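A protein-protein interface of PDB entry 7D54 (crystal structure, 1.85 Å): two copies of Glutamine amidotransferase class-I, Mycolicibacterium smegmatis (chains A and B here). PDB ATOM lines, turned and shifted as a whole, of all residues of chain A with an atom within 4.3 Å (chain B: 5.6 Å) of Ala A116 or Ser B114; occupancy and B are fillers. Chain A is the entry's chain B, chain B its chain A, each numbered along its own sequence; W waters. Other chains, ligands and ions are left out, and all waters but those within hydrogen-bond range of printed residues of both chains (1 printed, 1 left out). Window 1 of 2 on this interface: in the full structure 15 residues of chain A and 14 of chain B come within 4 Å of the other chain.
Water W1 bridges the backbone carbonyl oxygen of Val B115 (2.8 Å) and the guanidinium group of Arg A148 (3.1 Å).
Tyr A71 touches Gly B112.
CB of Ala A116 touches C of Gly B112, at 3.5 Å.
Gly B113 touches Ala A116.
Ala A116 touches Ser B114.
C of Gly B113 touches O of Arg A117, at 3.98 Å.
CD of Arg A117 touches CG2 of Thr B150, at 3.6 Å.
OG of Ser B114 touches CA of Ala A118 (3.5 Å).
Thr B150 touches Ala A118 (OG1 to C, 3.9 Å).
Val B115 touches Glu A119.
Ala B116 touches Glu A119.
The backbone NH (N) of Gly B113 lies within hydrogen-bond range of the backbone carbonyl oxygen (O) of Ala B108 (2.8 Å).
O of Ser B114 lies within hydrogen-bond range of N of Thr B150, 2.7 Å away.
The backbone NH of Arg B148 sits at hydrogen-bond distance from the backbone carbonyl oxygen of Ala B116, at 2.8 Å.
The backbone NH of Arg A148 sits at hydrogen-bond distance from the backbone carbonyl oxygen of Ala A116 (2.9 Å).
N of Arg A117 sits close to OD1 of Asp A147.
NH2 of Arg A148 lies within salt-bridge range of OE2 of Glu A119 (3.4 Å).
Hydrophobic or aromatic side chains of chain B within 4 Å of the printed part of chain A: Ala B116.
Among the printed residues, no Asp or Glu carboxylate lies within 4 Å of a Lys or Arg side-chain nitrogen of the other chain.
Of chain B, only Gly B112 (3.5 Å), Gly B113 (3.6 Å) and Ser B114 (3.4 Å) come within 4 Å of Ala A116.
Of the printed residues of chain A, Ser B114 touches Ala A116 (3.4 Å), Arg A117 (2.6 Å), Ala A118 (3.5 Å), Glu A119 (2.7 Å) and Arg A148 (3.2 Å).
Of the printed residues of chain B, Ala A118 touches Ser B114 (3.5 Å) and Thr B150 (3.9 Å).
Printed residues of chain B within 4 Å of Glu A119: Ser B114 (2.7 Å), Val B115 (3.8 Å), Ala B116 (3.4 Å) and Thr B150 (3.2 Å).
Of the printed residues of chain B, Arg A117 touches Gly B112 (2.8 Å), Gly B113 (3.98 Å), Ser B114 (2.6 Å) and Thr B150 (3.6 Å).
The nearest residue of chain B that does not touch Ala A116 is Gln B109 (4.9 Å).
The nearest printed residue of chain B that does not touch Arg A117 is Val B115 (5.6 Å).
N of Arg A117 is in hydrogen-bond range of O of Gly B112 (2.8 Å).
The backbone carbonyl oxygen of Arg A117 lies within hydrogen-bond range of the side-chain hydroxyl of Ser B114, at 2.6 Å.
OG of Ser B114 is in hydrogen-bond range of OE2 of Glu A119, at 2.7 Å.
The side-chain hydroxyl (OG) of Ser B114 sits close to the guanidinium group (NH2) of Arg A148 (3.3 Å).
O of Val B115 lies within hydrogen-bond range of NH2 of Arg A148, at 3.1 Å.
OG1 of Thr B150 sits close to OE2 of Glu A119.
Arg A148 touches Val B115, but with the chains exchanged Val A115 does not touch Arg B148 (12.9 Å).
Arg A148 touches Ala B116, but with the chains exchanged Ala A116 does not touch Arg B148 (10.0 Å).
3 positions are printed for both chains.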
ATOM      1  N   TYR A  71     -24.836  16.461  11.284  1.00  0.00           N
ATOM      2  CA  TYR A  71     -23.633  15.705  10.995  1.00  0.00           C
ATOM      3  C   TYR A  71     -23.903  14.516  10.065  1.00  0.00           C
ATOM      4  O   TYR A  71     -22.982  13.761   9.777  1.00  0.00           O
ATOM      5  CB  TYR A  71     -22.987  15.228  12.316  1.00  0.00           C
ATOM      6  CG  TYR A  71     -23.945  14.510  13.237  1.00  0.00           C
ATOM      7  CD1 TYR A  71     -24.199  13.149  13.075  1.00  0.00           C
ATOM      8  CD2 TYR A  71     -24.629  15.182  14.233  1.00  0.00           C
ATOM      9  CE1 TYR A  71     -25.107  12.486  13.894  1.00  0.00           C
ATOM     10  CE2 TYR A  71     -25.551  14.535  15.039  1.00  0.00           C
ATOM     11  CZ  TYR A  71     -25.774  13.181  14.867  1.00  0.00           C
ATOM     12  OH  TYR A  71     -26.689  12.540  15.677  1.00  0.00           O
ATOM     13  N   VAL A 115     -20.928  18.106  17.026  1.00  0.00           N
ATOM     14  CA  VAL A 115     -22.351  17.887  17.278  1.00  0.00           C
ATOM     15  C   VAL A 115     -22.584  16.387  17.290  1.00  0.00           C
ATOM     16  O   VAL A 115     -22.054  15.670  16.428  1.00  0.00           O
ATOM     17  CB  VAL A 115     -23.257  18.565  16.230  1.00  0.00           C
ATOM     18  CG1 VAL A 115     -24.731  18.361  16.596  1.00  0.00           C
ATOM     19  CG2 VAL A 115     -22.910  20.026  16.123  1.00  0.00           C
ATOM     20  N   ALA A 116     -23.335  15.904  18.289  1.00  0.00           N
ATOM     21  CA  ALA A 116     -23.542  14.467  18.394  1.00  0.00           C
ATOM     22  C   ALA A 116     -24.832  14.165  19.140  1.00  0.00           C
ATOM     23  O   ALA A 116     -25.353  15.002  19.883  1.00  0.00           O
ATOM     24  CB  ALA A 116     -22.372  13.768  19.089  1.00  0.00           C
ATOM     25  N   ARG A 117     -25.299  12.918  18.975  1.00  0.00           N
ATOM     26  CA  ARG A 117     -26.507  12.471  19.658  1.00  0.00           C
ATOM     27  C   ARG A 117     -26.344  12.521  21.166  1.00  0.00           C
ATOM     28  O   ARG A 117     -25.348  12.054  21.718  1.00  0.00           O
ATOM     29  CB  ARG A 117     -26.875  11.046  19.255  1.00  0.00           C
ATOM     30  CG  ARG A 117     -28.223  10.611  19.821  1.00  0.00           C
ATOM     31  CD  ARG A 117     -28.262   9.107  20.032  1.00  0.00           C
ATOM     32  NE  ARG A 117     -28.847   8.392  18.902  1.00  0.00           N
ATOM     33  CZ  ARG A 117     -28.192   7.504  18.166  1.00  0.00           C
ATOM     34  NH1 ARG A 117     -26.915   7.238  18.440  1.00  0.00           N
ATOM     35  NH2 ARG A 117     -28.806   6.898  17.161  1.00  0.00           N
ATOM     36  N   ALA A 118     -27.355  13.047  21.837  1.00  0.00           N
ATOM     37  CA  ALA A 118     -27.330  13.241  23.274  1.00  0.00           C
ATOM     38  C   ALA A 118     -27.828  12.007  24.016  1.00  0.00           C
ATOM     39  O   ALA A 118     -28.499  11.125  23.463  1.00  0.00           O
ATOM     40  CB  ALA A 118     -28.195  14.439  23.673  1.00  0.00           C
ATOM     41  N   GLU A 119     -27.477  11.966  25.292  1.00  0.00           N
ATOM     42  CA  GLU A 119     -27.927  10.899  26.174  1.00  0.00           C
ATOM     43  C   GLU A 119     -29.417  11.028  26.455  1.00  0.00           C
ATOM     44  O   GLU A 119     -30.188  10.085  26.221  1.00  0.00           O
ATOM     45  CB  GLU A 119     -27.117  10.956  27.466  1.00  0.00           C
ATOM     46  CG  GLU A 119     -25.587  10.949  27.277  1.00  0.00           C
ATOM     47  CD  GLU A 119     -24.968  12.213  26.606  1.00  0.00           C
ATOM     48  OE1 GLU A 119     -25.675  13.243  26.426  1.00  0.00           O
ATOM     49  OE2 GLU A 119     -23.753  12.166  26.251  1.00  0.00           O
ATOM     50  N   ASP A 147     -29.846  15.988  19.555  1.00  0.00           N
ATOM     51  CA  ASP A 147     -28.409  16.178  19.458  1.00  0.00           C
ATOM     52  C   ASP A 147     -27.983  17.365  20.314  1.00  0.00           C
ATOM     53  O   ASP A 147     -28.783  18.256  20.610  1.00  0.00           O
ATOM     54  CB  ASP A 147     -27.983  16.438  18.007  1.00  0.00           C
ATOM     55  CG  ASP A 147     -28.334  15.301  17.066  1.00  0.00           C
ATOM     56  OD1 ASP A 147     -27.984  14.135  17.337  1.00  0.00           O
ATOM     57  OD2 ASP A 147     -28.947  15.588  16.013  1.00  0.00           O
ATOM     58  N   ARG A 148     -26.690  17.410  20.651  1.00  0.00           N
ATOM     59  CA  ARG A 148     -26.118  18.488  21.459  1.00  0.00           C
ATOM     60  C   ARG A 148     -24.736  18.811  20.886  1.00  0.00           C
ATOM     61  O   ARG A 148     -24.084  17.966  20.264  1.00  0.00           O
ATOM     62  CB  ARG A 148     -25.936  18.066  22.918  1.00  0.00           C
ATOM     63  CG  ARG A 148     -24.864  16.983  22.907  1.00  0.00           C
ATOM     64  CD  ARG A 148     -24.847  15.980  23.995  1.00  0.00           C
ATOM     65  NE  ARG A 148     -24.596  16.506  25.316  1.00  0.00           N
ATOM     66  CZ  ARG A 148     -23.571  16.172  26.092  1.00  0.00           C
ATOM     67  NH1 ARG A 148     -23.505  16.698  27.307  1.00  0.00           N
ATOM     68  NH2 ARG A 148     -22.662  15.289  25.699  1.00  0.00           N
ATOM     69  N   ALA B 108     -16.824   7.162  19.535  1.00  0.00           N
ATOM     70  CA  ALA B 108     -18.226   7.508  19.631  1.00  0.00           C
ATOM     71  C   ALA B 108     -18.469   8.930  19.144  1.00  0.00           C
ATOM     72  O   ALA B 108     -19.348   9.169  18.311  1.00  0.00           O
ATOM     73  CB  ALA B 108     -18.690   7.306  21.067  1.00  0.00           C
ATOM     74  N   GLN B 109     -17.663   9.884  19.606  1.00  0.00           N
ATOM     75  CA  GLN B 109     -17.831  11.273  19.164  1.00  0.00           C
ATOM     76  C   GLN B 109     -17.580  11.421  17.662  1.00  0.00           C
ATOM     77  O   GLN B 109     -18.286  12.166  16.965  1.00  0.00           O
ATOM     78  CB  GLN B 109     -16.871  12.142  19.977  1.00  0.00           C
ATOM     79  CG  GLN B 109     -17.151  13.652  20.032  1.00  0.00           C
ATOM     80  CD  GLN B 109     -16.347  14.325  21.168  1.00  0.00           C
ATOM     81  OE1 GLN B 109     -16.865  14.571  22.256  1.00  0.00           O
ATOM     82  NE2 GLN B 109     -15.085  14.620  20.904  1.00  0.00           N
ATOM     83  N   GLY B 112     -20.805  10.458  15.831  1.00  0.00           N
ATOM     84  CA  GLY B 112     -22.055  11.113  16.153  1.00  0.00           C
ATOM     85  C   GLY B 112     -22.722  10.680  17.444  1.00  0.00           C
ATOM     86  O   GLY B 112     -23.909  10.948  17.611  1.00  0.00           O
ATOM     87  N   GLY B 113     -22.000  10.058  18.370  1.00  0.00           N
ATOM     88  CA  GLY B 113     -22.509   9.784  19.702  1.00  0.00           C
ATOM     89  C   GLY B 113     -21.774  10.615  20.729  1.00  0.00           C
ATOM     90  O   GLY B 113     -20.544  10.605  20.797  1.00  0.00           O
ATOM     91  N   SER B 114     -22.522  11.367  21.520  1.00  0.00           N
ATOM     92  CA  SER B 114     -21.843  12.276  22.421  1.00  0.00           C
ATOM     93  C   SER B 114     -21.330  11.555  23.670  1.00  0.00           C
ATOM     94  O   SER B 114     -21.695  10.418  23.966  1.00  0.00           O
ATOM     95  CB  SER B 114     -22.771  13.441  22.800  1.00  0.00           C
ATOM     96  OG  SER B 114     -23.830  12.989  23.629  1.00  0.00           O
ATOM     97  N   VAL B 115     -20.407  12.225  24.354  1.00  0.00           N
ATOM     98  CA  VAL B 115     -19.730  11.735  25.549  1.00  0.00           C
ATOM     99  C   VAL B 115     -19.967  12.735  26.663  1.00  0.00           C
ATOM    100  O   VAL B 115     -19.958  13.948  26.424  1.00  0.00           O
ATOM    101  CB  VAL B 115     -18.219  11.532  25.314  1.00  0.00           C
ATOM    102  CG1 VAL B 115     -17.543  11.077  26.556  1.00  0.00           C
ATOM    103  CG2 VAL B 115     -18.046  10.543  24.194  1.00  0.00           C
ATOM    104  N   ALA B 116     -20.184  12.226  27.871  1.00  0.00           N
ATOM    105  CA  ALA B 116     -20.551  13.098  28.973  1.00  0.00           C
ATOM    106  C   ALA B 116     -20.170  12.455  30.294  1.00  0.00           C
ATOM    107  O   ALA B 116     -19.982  11.235  30.398  1.00  0.00           O
ATOM    108  CB  ALA B 116     -22.054  13.406  28.962  1.00  0.00           C
ATOM    109  N   ARG B 148     -18.975   8.668  30.082  1.00  0.00           N
ATOM    110  CA  ARG B 148     -19.523   7.551  29.326  1.00  0.00           C
ATOM    111  C   ARG B 148     -19.999   8.058  27.972  1.00  0.00           C
ATOM    112  O   ARG B 148     -20.347   9.231  27.815  1.00  0.00           O
ATOM    113  CB  ARG B 148     -20.713   6.892  30.060  1.00  0.00           C
ATOM    114  CG  ARG B 148     -21.997   7.735  29.943  1.00  0.00           C
ATOM    115  CD  ARG B 148     -22.801   7.473  31.208  1.00  0.00           C
ATOM    116  NE  ARG B 148     -24.279   7.862  31.098  1.00  0.00           N
ATOM    117  CZ  ARG B 148     -25.331   7.119  31.458  1.00  0.00           C
ATOM    118  NH1 ARG B 148     -25.078   5.944  31.968  1.00  0.00           N
ATOM    119  NH2 ARG B 148     -26.585   7.551  31.308  1.00  0.00           N
ATOM    120  N   TRP B 149     -20.086   7.151  27.009  1.00  0.00           N
ATOM    121  CA  TRP B 149     -20.492   7.541  25.671  1.00  0.00           C
ATOM    122  C   TRP B 149     -21.943   7.178  25.394  1.00  0.00           C
ATOM    123  O   TRP B 149     -22.556   6.372  26.096  1.00  0.00           O
ATOM    124  CB  TRP B 149     -19.591   6.890  24.637  1.00  0.00           C
ATOM    125  CG  TRP B 149     -19.707   5.371  24.501  1.00  0.00           C
ATOM    126  CD1 TRP B 149     -20.824   4.645  24.282  1.00  0.00           C
ATOM    127  CD2 TRP B 149     -18.616   4.440  24.512  1.00  0.00           C
ATOM    128  NE1 TRP B 149     -20.500   3.305  24.137  1.00  0.00           N
ATOM    129  CE2 TRP B 149     -19.151   3.158  24.304  1.00  0.00           C
ATOM    130  CE3 TRP B 149     -17.228   4.575  24.688  1.00  0.00           C
ATOM    131  CZ2 TRP B 149     -18.353   2.022  24.268  1.00  0.00           C
ATOM    132  CZ3 TRP B 149     -16.446   3.484  24.659  1.00  0.00           C
ATOM    133  CH2 TRP B 149     -17.003   2.196  24.457  1.00  0.00           C
ATOM    134  N   THR B 150     -22.494   7.837  24.373  1.00  0.00           N
ATOM    135  CA  THR B 150     -23.760   7.484  23.747  1.00  0.00           C
ATOM    136  C   THR B 150     -23.387   6.715  22.488  1.00  0.00           C
ATOM    137  O   THR B 150     -22.626   7.236  21.651  1.00  0.00           O
ATOM    138  CB  THR B 150     -24.579   8.730  23.393  1.00  0.00           C
ATOM    139  OG1 THR B 150     -24.973   9.397  24.603  1.00  0.00           O
ATOM    140  CG2 THR B 150     -25.808   8.302  22.575  1.00  0.00           C
HETATM  141  O   HOH W   1     -20.379  16.567  27.458  1.00  0.00           O
